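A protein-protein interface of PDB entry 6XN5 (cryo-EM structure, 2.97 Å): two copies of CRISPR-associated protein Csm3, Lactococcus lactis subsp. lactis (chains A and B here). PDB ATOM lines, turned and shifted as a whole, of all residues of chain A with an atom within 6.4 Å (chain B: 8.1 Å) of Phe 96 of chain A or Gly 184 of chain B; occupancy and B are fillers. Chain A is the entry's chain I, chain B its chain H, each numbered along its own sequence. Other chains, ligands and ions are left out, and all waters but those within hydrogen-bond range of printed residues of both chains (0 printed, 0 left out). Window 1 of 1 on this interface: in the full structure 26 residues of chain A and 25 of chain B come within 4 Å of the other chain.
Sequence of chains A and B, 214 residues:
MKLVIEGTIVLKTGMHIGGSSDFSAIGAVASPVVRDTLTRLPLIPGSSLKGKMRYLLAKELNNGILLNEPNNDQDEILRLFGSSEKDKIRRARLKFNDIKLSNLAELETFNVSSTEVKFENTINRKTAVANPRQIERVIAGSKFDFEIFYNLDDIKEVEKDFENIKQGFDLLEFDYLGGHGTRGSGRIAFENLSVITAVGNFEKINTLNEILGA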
ATOM      1  N   PRO A  45       0.113  -7.915  -7.560  1.00  0.00           N
ATOM      2  CA  PRO A  45       0.293  -6.508  -7.211  1.00  0.00           C
ATOM      3  C   PRO A  45       1.753  -6.213  -6.934  1.00  0.00           C
ATOM      4  O   PRO A  45       2.496  -7.070  -6.458  1.00  0.00           O
ATOM      5  CB  PRO A  45      -0.561  -6.344  -5.952  1.00  0.00           C
ATOM      6  CG  PRO A  45      -1.511  -7.469  -5.981  1.00  0.00           C
ATOM      7  CD  PRO A  45      -0.798  -8.597  -6.633  1.00  0.00           C
ATOM      8  N   GLY A  46       2.168  -4.990  -7.246  1.00  0.00           N
ATOM      9  CA  GLY A  46       3.493  -4.564  -6.846  1.00  0.00           C
ATOM     10  C   GLY A  46       3.596  -4.369  -5.350  1.00  0.00           C
ATOM     11  O   GLY A  46       4.687  -4.452  -4.779  1.00  0.00           O
ATOM     12  N   SER A  47       2.460  -4.121  -4.697  1.00  0.00           N
ATOM     13  CA  SER A  47       2.429  -4.017  -3.245  1.00  0.00           C
ATOM     14  C   SER A  47       2.737  -5.351  -2.593  1.00  0.00           C
ATOM     15  O   SER A  47       3.487  -5.422  -1.615  1.00  0.00           O
ATOM     16  CB  SER A  47       1.068  -3.504  -2.794  1.00  0.00           C
ATOM     17  OG  SER A  47       1.009  -3.425  -1.384  1.00  0.00           O
ATOM     18  N   LEU A  49       4.382  -7.905  -4.035  1.00  0.00           N
ATOM     19  CA  LEU A  49       5.765  -8.258  -4.325  1.00  0.00           C
ATOM     20  C   LEU A  49       6.721  -7.478  -3.445  1.00  0.00           C
ATOM     21  O   LEU A  49       7.681  -8.047  -2.920  1.00  0.00           O
ATOM     22  CB  LEU A  49       6.093  -8.026  -5.795  1.00  0.00           C
ATOM     23  CG  LEU A  49       7.422  -8.679  -6.173  1.00  0.00           C
ATOM     24  CD1 LEU A  49       7.331 -10.178  -6.026  1.00  0.00           C
ATOM     25  CD2 LEU A  49       7.838  -8.317  -7.571  1.00  0.00           C
ATOM     26  N   LYS A  50       6.437  -6.190  -3.221  1.00  0.00           N
ATOM     27  CA  LYS A  50       7.251  -5.396  -2.306  1.00  0.00           C
ATOM     28  C   LYS A  50       7.184  -5.921  -0.877  1.00  0.00           C
ATOM     29  O   LYS A  50       8.214  -6.018  -0.203  1.00  0.00           O
ATOM     30  CB  LYS A  50       6.815  -3.936  -2.321  1.00  0.00           C
ATOM     31  CG  LYS A  50       7.731  -3.099  -1.467  1.00  0.00           C
ATOM     32  CD  LYS A  50       7.322  -1.679  -1.377  1.00  0.00           C
ATOM     33  CE  LYS A  50       7.595  -0.939  -2.612  1.00  0.00           C
ATOM     34  NZ  LYS A  50       7.250   0.464  -2.327  1.00  0.00           N
ATOM     35  N   MET A  53       8.900  -9.335  -0.619  1.00  0.00           N
ATOM     36  CA  MET A  53      10.307  -9.084  -0.896  1.00  0.00           C
ATOM     37  C   MET A  53      11.006  -8.478   0.315  1.00  0.00           C
ATOM     38  O   MET A  53      12.070  -8.952   0.732  1.00  0.00           O
ATOM     39  CB  MET A  53      10.361  -8.141  -2.097  1.00  0.00           C
ATOM     40  CG  MET A  53      11.674  -7.787  -2.758  1.00  0.00           C
ATOM     41  SD  MET A  53      12.534  -9.117  -3.593  1.00  0.00           S
ATOM     42  CE  MET A  53      14.186  -8.456  -3.558  1.00  0.00           C
ATOM     43  N   PHE A  81      13.541   0.383  -0.101  1.00  0.00           N
ATOM     44  CA  PHE A  81      12.090   0.281  -0.106  1.00  0.00           C
ATOM     45  C   PHE A  81      11.403   1.480   0.535  1.00  0.00           C
ATOM     46  O   PHE A  81      10.180   1.592   0.448  1.00  0.00           O
ATOM     47  CB  PHE A  81      11.651  -0.997   0.603  1.00  0.00           C
ATOM     48  CG  PHE A  81      12.001  -2.248  -0.135  1.00  0.00           C
ATOM     49  CD1 PHE A  81      11.379  -2.559  -1.334  1.00  0.00           C
ATOM     50  CD2 PHE A  81      12.920  -3.138   0.383  1.00  0.00           C
ATOM     51  CE1 PHE A  81      11.692  -3.717  -2.008  1.00  0.00           C
ATOM     52  CE2 PHE A  81      13.234  -4.298  -0.286  1.00  0.00           C
ATOM     53  CZ  PHE A  81      12.621  -4.582  -1.487  1.00  0.00           C
ATOM     54  N   LEU A  94      13.242   2.426  -4.919  1.00  0.00           N
ATOM     55  CA  LEU A  94      12.840   1.256  -5.689  1.00  0.00           C
ATOM     56  C   LEU A  94      11.340   1.304  -5.943  1.00  0.00           C
ATOM     57  O   LEU A  94      10.548   1.296  -4.997  1.00  0.00           O
ATOM     58  CB  LEU A  94      13.228  -0.033  -4.958  1.00  0.00           C
ATOM     59  CG  LEU A  94      13.220  -1.328  -5.766  1.00  0.00           C
ATOM     60  CD1 LEU A  94      14.297  -1.291  -6.821  1.00  0.00           C
ATOM     61  CD2 LEU A  94      13.452  -2.503  -4.865  1.00  0.00           C
ATOM     62  N   LYS A  95      10.955   1.339  -7.218  1.00  0.00           N
ATOM     63  CA  LYS A  95       9.567   1.510  -7.627  1.00  0.00           C
ATOM     64  C   LYS A  95       9.089   0.237  -8.306  1.00  0.00           C
ATOM     65  O   LYS A  95       9.622  -0.148  -9.349  1.00  0.00           O
ATOM     66  CB  LYS A  95       9.425   2.704  -8.576  1.00  0.00           C
ATOM     67  CG  LYS A  95       7.999   3.182  -8.811  1.00  0.00           C
ATOM     68  CD  LYS A  95       7.409   2.658 -10.108  1.00  0.00           C
ATOM     69  CE  LYS A  95       6.016   3.199 -10.326  1.00  0.00           C
ATOM     70  NZ  LYS A  95       5.304   2.520 -11.428  1.00  0.00           N
ATOM     71  N   PHE A  96       8.066  -0.389  -7.736  1.00  0.00           N
ATOM     72  CA  PHE A  96       7.449  -1.576  -8.303  1.00  0.00           C
ATOM     73  C   PHE A  96       6.243  -1.199  -9.150  1.00  0.00           C
ATOM     74  O   PHE A  96       5.686  -0.108  -9.036  1.00  0.00           O
ATOM     75  CB  PHE A  96       7.017  -2.534  -7.204  1.00  0.00           C
ATOM     76  CG  PHE A  96       8.139  -3.290  -6.600  1.00  0.00           C
ATOM     77  CD1 PHE A  96       8.580  -4.469  -7.163  1.00  0.00           C
ATOM     78  CD2 PHE A  96       8.764  -2.814  -5.468  1.00  0.00           C
ATOM     79  CE1 PHE A  96       9.620  -5.167  -6.594  1.00  0.00           C
ATOM     80  CE2 PHE A  96       9.799  -3.503  -4.897  1.00  0.00           C
ATOM     81  CZ  PHE A  96      10.230  -4.682  -5.460  1.00  0.00           C
ATOM     82  N   ASN A  97       5.831  -2.132  -9.998  1.00  0.00           N
ATOM     83  CA  ASN A  97       4.709  -1.924 -10.893  1.00  0.00           C
ATOM     84  C   ASN A  97       3.774  -3.114 -10.810  1.00  0.00           C
ATOM     85  O   ASN A  97       4.188  -4.222 -10.469  1.00  0.00           O
ATOM     86  CB  ASN A  97       5.174  -1.732 -12.331  1.00  0.00           C
ATOM     87  CG  ASN A  97       6.198  -0.633 -12.466  1.00  0.00           C
ATOM     88  OD1 ASN A  97       5.852   0.525 -12.678  1.00  0.00           O
ATOM     89  ND2 ASN A  97       7.464  -0.983 -12.323  1.00  0.00           N
ATOM     90  N   ASP A  98       2.508  -2.868 -11.125  1.00  0.00           N
ATOM     91  CA  ASP A  98       1.507  -3.921 -11.081  1.00  0.00           C
ATOM     92  C   ASP A  98       1.764  -4.931 -12.183  1.00  0.00           C
ATOM     93  O   ASP A  98       1.579  -4.640 -13.366  1.00  0.00           O
ATOM     94  CB  ASP A  98       0.111  -3.325 -11.214  1.00  0.00           C
ATOM     95  CG  ASP A  98      -0.461  -2.901  -9.884  1.00  0.00           C
ATOM     96  OD1 ASP A  98       0.011  -3.410  -8.848  1.00  0.00           O
ATOM     97  OD2 ASP A  98      -1.378  -2.054  -9.873  1.00  0.00           O
ATOM     98  N   ILE A  99       2.199  -6.109 -11.781  1.00  0.00           N
ATOM     99  CA  ILE A  99       2.626  -7.153 -12.696  1.00  0.00           C
ATOM    100  C   ILE A  99       1.390  -7.838 -13.251  1.00  0.00           C
ATOM    101  O   ILE A  99       0.592  -8.389 -12.491  1.00  0.00           O
ATOM    102  CB  ILE A  99       3.514  -8.165 -11.963  1.00  0.00           C
ATOM    103  CG1 ILE A  99       4.759  -7.490 -11.410  1.00  0.00           C
ATOM    104  CG2 ILE A  99       3.921  -9.249 -12.900  1.00  0.00           C
ATOM    105  CD1 ILE A  99       5.513  -8.363 -10.467  1.00  0.00           C
ATOM    106  N   GLU A 147       8.778  -4.836 -14.696  1.00  0.00           N
ATOM    107  CA  GLU A 147       9.752  -3.790 -15.025  1.00  0.00           C
ATOM    108  C   GLU A 147       9.897  -2.897 -13.797  1.00  0.00           C
ATOM    109  O   GLU A 147       9.208  -1.885 -13.672  1.00  0.00           O
ATOM    110  CB  GLU A 147       9.329  -2.984 -16.248  1.00  0.00           C
ATOM    111  CG  GLU A 147       9.231  -3.775 -17.547  1.00  0.00           C
ATOM    112  CD  GLU A 147       9.385  -2.899 -18.781  1.00  0.00           C
ATOM    113  OE1 GLU A 147       9.352  -3.438 -19.906  1.00  0.00           O
ATOM    114  OE2 GLU A 147       9.546  -1.671 -18.627  1.00  0.00           O
ATOM    115  N   ILE A 148      10.807  -3.265 -12.907  1.00  0.00           N
ATOM    116  CA  ILE A 148      11.078  -2.485 -11.707  1.00  0.00           C
ATOM    117  C   ILE A 148      11.979  -1.317 -12.082  1.00  0.00           C
ATOM    118  O   ILE A 148      13.044  -1.513 -12.674  1.00  0.00           O
ATOM    119  CB  ILE A 148      11.726  -3.352 -10.620  1.00  0.00           C
ATOM    120  CG1 ILE A 148      10.868  -4.581 -10.336  1.00  0.00           C
ATOM    121  CG2 ILE A 148      11.935  -2.552  -9.362  1.00  0.00           C
ATOM    122  CD1 ILE A 148      11.639  -5.733  -9.748  1.00  0.00           C
ATOM    123  N   PHE A 149      11.558  -0.104 -11.739  1.00  0.00           N
ATOM    124  CA  PHE A 149      12.338   1.084 -12.047  1.00  0.00           C
ATOM    125  C   PHE A 149      13.299   1.390 -10.913  1.00  0.00           C
ATOM    126  O   PHE A 149      12.937   1.336  -9.736  1.00  0.00           O
ATOM    127  CB  PHE A 149      11.440   2.300 -12.265  1.00  0.00           C
ATOM    128  CG  PHE A 149      10.427   2.134 -13.351  1.00  0.00           C
ATOM    129  CD1 PHE A 149      10.682   1.341 -14.454  1.00  0.00           C
ATOM    130  CD2 PHE A 149       9.216   2.792 -13.271  1.00  0.00           C
ATOM    131  CE1 PHE A 149       9.747   1.200 -15.446  1.00  0.00           C
ATOM    132  CE2 PHE A 149       8.277   2.654 -14.260  1.00  0.00           C
ATOM    133  CZ  PHE A 149       8.542   1.859 -15.349  1.00  0.00           C
ATOM    134  N   PHE A 169      15.583 -12.178  -4.560  1.00  0.00           N
ATOM    135  CA  PHE A 169      14.934 -13.078  -5.512  1.00  0.00           C
ATOM    136  C   PHE A 169      15.331 -14.527  -5.232  1.00  0.00           C
ATOM    137  O   PHE A 169      14.500 -15.450  -5.309  1.00  0.00           O
ATOM    138  CB  PHE A 169      15.292 -12.690  -6.947  1.00  0.00           C
ATOM    139  CG  PHE A 169      14.723 -11.365  -7.393  1.00  0.00           C
ATOM    140  CD1 PHE A 169      13.668 -10.767  -6.722  1.00  0.00           C
ATOM    141  CD2 PHE A 169      15.222 -10.739  -8.529  1.00  0.00           C
ATOM    142  CE1 PHE A 169      13.148  -9.561  -7.150  1.00  0.00           C
ATOM    143  CE2 PHE A 169      14.702  -9.539  -8.965  1.00  0.00           C
ATOM    144  CZ  PHE A 169      13.667  -8.950  -8.274  1.00  0.00           C
ATOM    145  N   LYS B  12      -0.481   3.053 -17.367  1.00  0.00           N
ATOM    146  CA  LYS B  12      -0.052   1.680 -17.573  1.00  0.00           C
ATOM    147  C   LYS B  12      -0.414   0.777 -16.404  1.00  0.00           C
ATOM    148  O   LYS B  12      -0.793  -0.379 -16.619  1.00  0.00           O
ATOM    149  CB  LYS B  12       1.455   1.632 -17.833  1.00  0.00           C
ATOM    150  CG  LYS B  12       1.904   2.484 -19.009  1.00  0.00           C
ATOM    151  CD  LYS B  12       1.170   2.123 -20.293  1.00  0.00           C
ATOM    152  CE  LYS B  12       1.534   0.733 -20.793  1.00  0.00           C
ATOM    153  NZ  LYS B  12       2.960   0.628 -21.194  1.00  0.00           N
ATOM    154  N   THR B  13      -0.307   1.277 -15.176  1.00  0.00           N
ATOM    155  CA  THR B  13      -0.814   0.578 -14.002  1.00  0.00           C
ATOM    156  C   THR B  13      -1.930   1.412 -13.398  1.00  0.00           C
ATOM    157  O   THR B  13      -2.404   2.357 -14.031  1.00  0.00           O
ATOM    158  CB  THR B  13       0.280   0.338 -12.963  1.00  0.00           C
ATOM    159  OG1 THR B  13       0.604   1.572 -12.321  1.00  0.00           O
ATOM    160  CG2 THR B  13       1.520  -0.232 -13.604  1.00  0.00           C
ATOM    161  N   GLY B  14      -2.381   1.063 -12.207  1.00  0.00           N
ATOM    162  CA  GLY B  14      -3.375   1.870 -11.539  1.00  0.00           C
ATOM    163  C   GLY B  14      -2.798   3.185 -11.057  1.00  0.00           C
ATOM    164  O   GLY B  14      -1.588   3.386 -10.989  1.00  0.00           O
ATOM    165  N   MET B  15      -3.693   4.109 -10.726  1.00  0.00           N
ATOM    166  CA  MET B  15      -3.279   5.405 -10.218  1.00  0.00           C
ATOM    167  C   MET B  15      -4.238   5.803  -9.115  1.00  0.00           C
ATOM    168  O   MET B  15      -5.371   5.336  -9.068  1.00  0.00           O
ATOM    169  CB  MET B  15      -3.249   6.463 -11.325  1.00  0.00           C
ATOM    170  CG  MET B  15      -2.414   7.698 -11.022  1.00  0.00           C
ATOM    171  SD  MET B  15      -2.603   8.954 -12.281  1.00  0.00           S
ATOM    172  CE  MET B  15      -4.332   9.332 -12.070  1.00  0.00           C
ATOM    173  N   LYS B 118      -8.955  -1.222  -4.157  1.00  0.00           N
ATOM    174  CA  LYS B 118      -7.819  -2.122  -4.021  1.00  0.00           C
ATOM    175  C   LYS B 118      -7.651  -2.479  -2.554  1.00  0.00           C
ATOM    176  O   LYS B 118      -7.455  -1.595  -1.716  1.00  0.00           O
ATOM    177  CB  LYS B 118      -6.546  -1.471  -4.555  1.00  0.00           C
ATOM    178  CG  LYS B 118      -5.292  -2.251  -4.238  1.00  0.00           C
ATOM    179  CD  LYS B 118      -4.061  -1.454  -4.561  1.00  0.00           C
ATOM    180  CE  LYS B 118      -2.817  -2.182  -4.116  1.00  0.00           C
ATOM    181  NZ  LYS B 118      -1.602  -1.359  -4.353  1.00  0.00           N
ATOM    182  N   ARG B 137      -8.574   3.254  -6.493  1.00  0.00           N
ATOM    183  CA  ARG B 137      -7.677   3.558  -7.596  1.00  0.00           C
ATOM    184  C   ARG B 137      -8.470   3.692  -8.882  1.00  0.00           C
ATOM    185  O   ARG B 137      -9.338   2.871  -9.175  1.00  0.00           O
ATOM    186  CB  ARG B 137      -6.589   2.489  -7.797  1.00  0.00           C
ATOM    187  CG  ARG B 137      -5.699   2.241  -6.602  1.00  0.00           C
ATOM    188  CD  ARG B 137      -4.422   1.543  -6.997  1.00  0.00           C
ATOM    189  NE  ARG B 137      -4.638   0.521  -8.010  1.00  0.00           N
ATOM    190  CZ  ARG B 137      -3.682  -0.279  -8.465  1.00  0.00           C
ATOM    191  NH1 ARG B 137      -2.452  -0.172  -7.991  1.00  0.00           N
ATOM    192  NH2 ARG B 137      -3.957  -1.186  -9.387  1.00  0.00           N
ATOM    193  N   TYR B 176       6.320   7.439 -11.678  1.00  0.00           N
ATOM    194  CA  TYR B 176       4.889   7.416 -11.431  1.00  0.00           C
ATOM    195  C   TYR B 176       4.318   8.817 -11.279  1.00  0.00           C
ATOM    196  O   TYR B 176       5.026   9.824 -11.323  1.00  0.00           O
ATOM    197  CB  TYR B 176       4.557   6.567 -10.201  1.00  0.00           C
ATOM    198  CG  TYR B 176       5.112   7.045  -8.881  1.00  0.00           C
ATOM    199  CD1 TYR B 176       6.357   6.620  -8.449  1.00  0.00           C
ATOM    200  CD2 TYR B 176       4.392   7.899  -8.059  1.00  0.00           C
ATOM    201  CE1 TYR B 176       6.872   7.027  -7.248  1.00  0.00           C
ATOM    202  CE2 TYR B 176       4.898   8.309  -6.853  1.00  0.00           C
ATOM    203  CZ  TYR B 176       6.140   7.872  -6.454  1.00  0.00           C
ATOM    204  OH  TYR B 176       6.661   8.281  -5.250  1.00  0.00           O
ATOM    205  N   GLY B 178       1.759  10.387  -8.627  1.00  0.00           N
ATOM    206  CA  GLY B 178       0.901  10.564  -7.473  1.00  0.00           C
ATOM    207  C   GLY B 178       0.414   9.314  -6.773  1.00  0.00           C
ATOM    208  O   GLY B 178       0.109   8.300  -7.404  1.00  0.00           O
ATOM    209  N   GLY B 179       0.307   9.391  -5.455  1.00  0.00           N
ATOM    210  CA  GLY B 179      -0.160   8.281  -4.659  1.00  0.00           C
ATOM    211  C   GLY B 179       0.924   7.274  -4.373  1.00  0.00           C
ATOM    212  O   GLY B 179       2.106   7.508  -4.605  1.00  0.00           O
ATOM    213  N   HIS B 180       0.490   6.101  -3.912  1.00  0.00           N
ATOM    214  CA  HIS B 180       1.387   5.055  -3.438  1.00  0.00           C
ATOM    215  C   HIS B 180       2.155   4.453  -4.599  1.00  0.00           C
ATOM    216  O   HIS B 180       1.875   3.332  -5.032  1.00  0.00           O
ATOM    217  CB  HIS B 180       0.600   3.963  -2.731  1.00  0.00           C
ATOM    218  CG  HIS B 180      -0.458   4.477  -1.813  1.00  0.00           C
ATOM    219  ND1 HIS B 180      -1.779   4.571  -2.185  1.00  0.00           N
ATOM    220  CD2 HIS B 180      -0.392   4.917  -0.536  1.00  0.00           C
ATOM    221  CE1 HIS B 180      -2.482   5.049  -1.174  1.00  0.00           C
ATOM    222  NE2 HIS B 180      -1.663   5.268  -0.163  1.00  0.00           N
ATOM    223  N   GLY B 181       3.142   5.192  -5.091  1.00  0.00           N
ATOM    224  CA  GLY B 181       3.643   4.926  -6.420  1.00  0.00           C
ATOM    225  C   GLY B 181       4.646   3.802  -6.465  1.00  0.00           C
ATOM    226  O   GLY B 181       4.627   2.981  -7.383  1.00  0.00           O
ATOM    227  N   THR B 182       5.524   3.735  -5.468  1.00  0.00           N
ATOM    228  CA  THR B 182       6.554   2.711  -5.448  1.00  0.00           C
ATOM    229  C   THR B 182       5.990   1.321  -5.207  1.00  0.00           C
ATOM    230  O   THR B 182       6.694   0.337  -5.440  1.00  0.00           O
ATOM    231  CB  THR B 182       7.586   3.054  -4.384  1.00  0.00           C
ATOM    232  OG1 THR B 182       6.983   2.953  -3.091  1.00  0.00           O
ATOM    233  CG2 THR B 182       8.109   4.464  -4.585  1.00  0.00           C
ATOM    234  N   ARG B 183       4.721   1.225  -4.827  1.00  0.00           N
ATOM    235  CA  ARG B 183       4.081   0.007  -4.372  1.00  0.00           C
ATOM    236  C   ARG B 183       3.097  -0.509  -5.415  1.00  0.00           C
ATOM    237  O   ARG B 183       2.156  -1.226  -5.090  1.00  0.00           O
ATOM    238  CB  ARG B 183       3.377   0.296  -3.052  1.00  0.00           C
ATOM    239  CG  ARG B 183       3.422  -0.777  -2.028  1.00  0.00           C
ATOM    240  CD  ARG B 183       2.972  -0.232  -0.707  1.00  0.00           C
ATOM    241  NE  ARG B 183       3.754   0.947  -0.371  1.00  0.00           N
ATOM    242  CZ  ARG B 183       3.223   2.142  -0.153  1.00  0.00           C
ATOM    243  NH1 ARG B 183       1.912   2.295  -0.190  1.00  0.00           N
ATOM    244  NH2 ARG B 183       4.004   3.169   0.134  1.00  0.00           N
ATOM    245  N   GLY B 184       3.290  -0.128  -6.673  1.00  0.00           N
ATOM    246  CA  GLY B 184       2.439  -0.608  -7.743  1.00  0.00           C
ATOM    247  C   GLY B 184       1.734   0.468  -8.544  1.00  0.00           C
ATOM    248  O   GLY B 184       1.578   0.340  -9.760  1.00  0.00           O
ATOM    249  N   SER B 185       1.312   1.537  -7.881  1.00  0.00           N
ATOM    250  CA  SER B 185       0.446   2.513  -8.519  1.00  0.00           C
ATOM    251  C   SER B 185       1.247   3.513  -9.344  1.00  0.00           C
ATOM    252  O   SER B 185       2.459   3.657  -9.194  1.00  0.00           O
ATOM    253  CB  SER B 185      -0.363   3.268  -7.471  1.00  0.00           C
ATOM    254  OG  SER B 185      -1.127   2.380  -6.684  1.00  0.00           O
ATOM    255  N   GLY B 186       0.544   4.200 -10.245  1.00  0.00           N
ATOM    256  CA  GLY B 186       0.985   5.482 -10.745  1.00  0.00           C
ATOM    257  C   GLY B 186       1.682   5.503 -12.088  1.00  0.00           C
ATOM    258  O   GLY B 186       1.942   6.597 -12.599  1.00  0.00           O
ATOM    259  N   ARG B 187       1.998   4.354 -12.678  1.00  0.00           N
ATOM    260  CA  ARG B 187       2.822   4.350 -13.880  1.00  0.00           C
ATOM    261  C   ARG B 187       2.038   4.841 -15.088  1.00  0.00           C
ATOM    262  O   ARG B 187       1.009   4.269 -15.452  1.00  0.00           O
ATOM    263  CB  ARG B 187       3.368   2.956 -14.154  1.00  0.00           C
ATOM    264  CG  ARG B 187       4.273   2.914 -15.362  1.00  0.00           C
ATOM    265  CD  ARG B 187       4.728   1.513 -15.689  1.00  0.00           C
ATOM    266  NE  ARG B 187       5.622   1.500 -16.840  1.00  0.00           N
ATOM    267  CZ  ARG B 187       6.026   0.397 -17.457  1.00  0.00           C
ATOM    268  NH1 ARG B 187       5.617  -0.788 -17.035  1.00  0.00           N
ATOM    269  NH2 ARG B 187       6.842   0.480 -18.495  1.00  0.00           N
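Printed residues of chain B that touch a printed residue of chain A: Thr 13, Lys 118, Arg 137, Tyr 176, Gly 181, Thr 182, Arg 183, Gly 184, Ser 185 and Arg 187.
Hydrophobic or aromatic side chains of chain B that line the printed part of chain A: Tyr 176.
Hydrophobic or aromatic side chains of chain A that line the printed part of chain B: Phe 96 and Phe 149.
No position is printed for both chains.
The backbone NH of Lys 12 of chain B lies within hydrogen-bond range of the backbone carbonyl oxygen of Arg 187 of chain B.
The side-chain amino group (NZ) of Lys 95 of chain A is in hydrogen-bond range of the side-chain amide oxygen (OD1) of Asn 97 of chain A (2.4 Å).
The backbone NH (N) of Phe 149 of chain A lies within hydrogen-bond range of the backbone carbonyl oxygen (O) of Lys 95 of chain A, 3.1 Å away.
The side-chain hydroxyl (OG1) of Thr 13 of chain B is in hydrogen-bond range of the backbone NH (N) of Gly 186 of chain B.
The guanidinium group of Arg 137 of chain B is in hydrogen-bond range of the side-chain hydroxyl of Ser 185 of chain B (3.2 Å).
OG1 of Thr 13 of chain B is in hydrogen-bond range of N of Arg 187 of chain B, 3.1 Å away.
Lys 118 of chain B touches Ser 47 of chain A (NZ to CB, 3.8 Å).
NZ of Lys 50 of chain A touches N of Arg 183 of chain B, 3.6 Å away.
Thr 182 of chain B touches Leu 94 of chain A (CB to O, 3.5 Å).
O of Gly 181 of chain B touches CE of Lys 95 of chain A (3.3 Å).
Thr 182 of chain B touches Lys 95 of chain A (CA to CG, 3.7 Å).
NZ of Lys 95 of chain A touches CB of Arg 187 of chain B, at 3.4 Å.
Phe 96 of chain A touches Gly 181 of chain B.
OD1 of Asn 97 of chain A touches CD of Arg 187 of chain B, at 3.4 Å.
N of Asp 98 of chain A touches O of Gly 184 of chain B (3.6 Å).
Phe 149 of chain A touches Arg 187 of chain B.
Printed residues of chain B within 4 Å of Asn 97 of chain A: Arg 187.
Met 15 of chain B touches none of the printed residues of chain A.
Printed residues of chain A within 4 Å of Lys 118 of chain B: Ser 47.
Gly 179 of chain B touches none of the printed residues of chain A.
Of the printed residues of chain A, Arg 183 of chain B touches Gly 46, Ser 47 and Lys 50.
Of the printed residues of chain A, Ser 185 of chain B touches Lys 95 (3.8 Å).
The nearest residue of chain A that does not touch Gly 184 of chain B is Asn 97 of chain A (4.03 Å).
The nearest printed residue of chain A that does not touch Thr 182 of chain B is Phe 81 of chain A (5.0 Å).
The side-chain hydroxyl (OG1) of Thr 182 of chain B sits at hydrogen-bond distance from the side-chain amino group (NZ) of Lys 50 of chain A (2.6 Å).
NH2 of Arg 137 of chain B is in salt-bridge range of OD2 of Asp 98 of chain A (2.8 Å).
The backbone carbonyl oxygen (O) of Phe 96 of chain A lies within hydrogen-bond range of the backbone NH (N) of Gly 184 of chain B (3.4 Å).
The backbone NH of Ser 47 of chain A is in hydrogen-bond range of the backbone carbonyl oxygen of Arg 183 of chain B, 2.9 Å away.
The backbone NH (N) of Phe 96 of chain A sits at hydrogen-bond distance from the backbone carbonyl oxygen (O) of Thr 182 of chain B (2.8 Å).
NH2 of Arg 187 of chain B is in salt-bridge range of OE2 of Glu 147 of chain A (3.5 Å).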
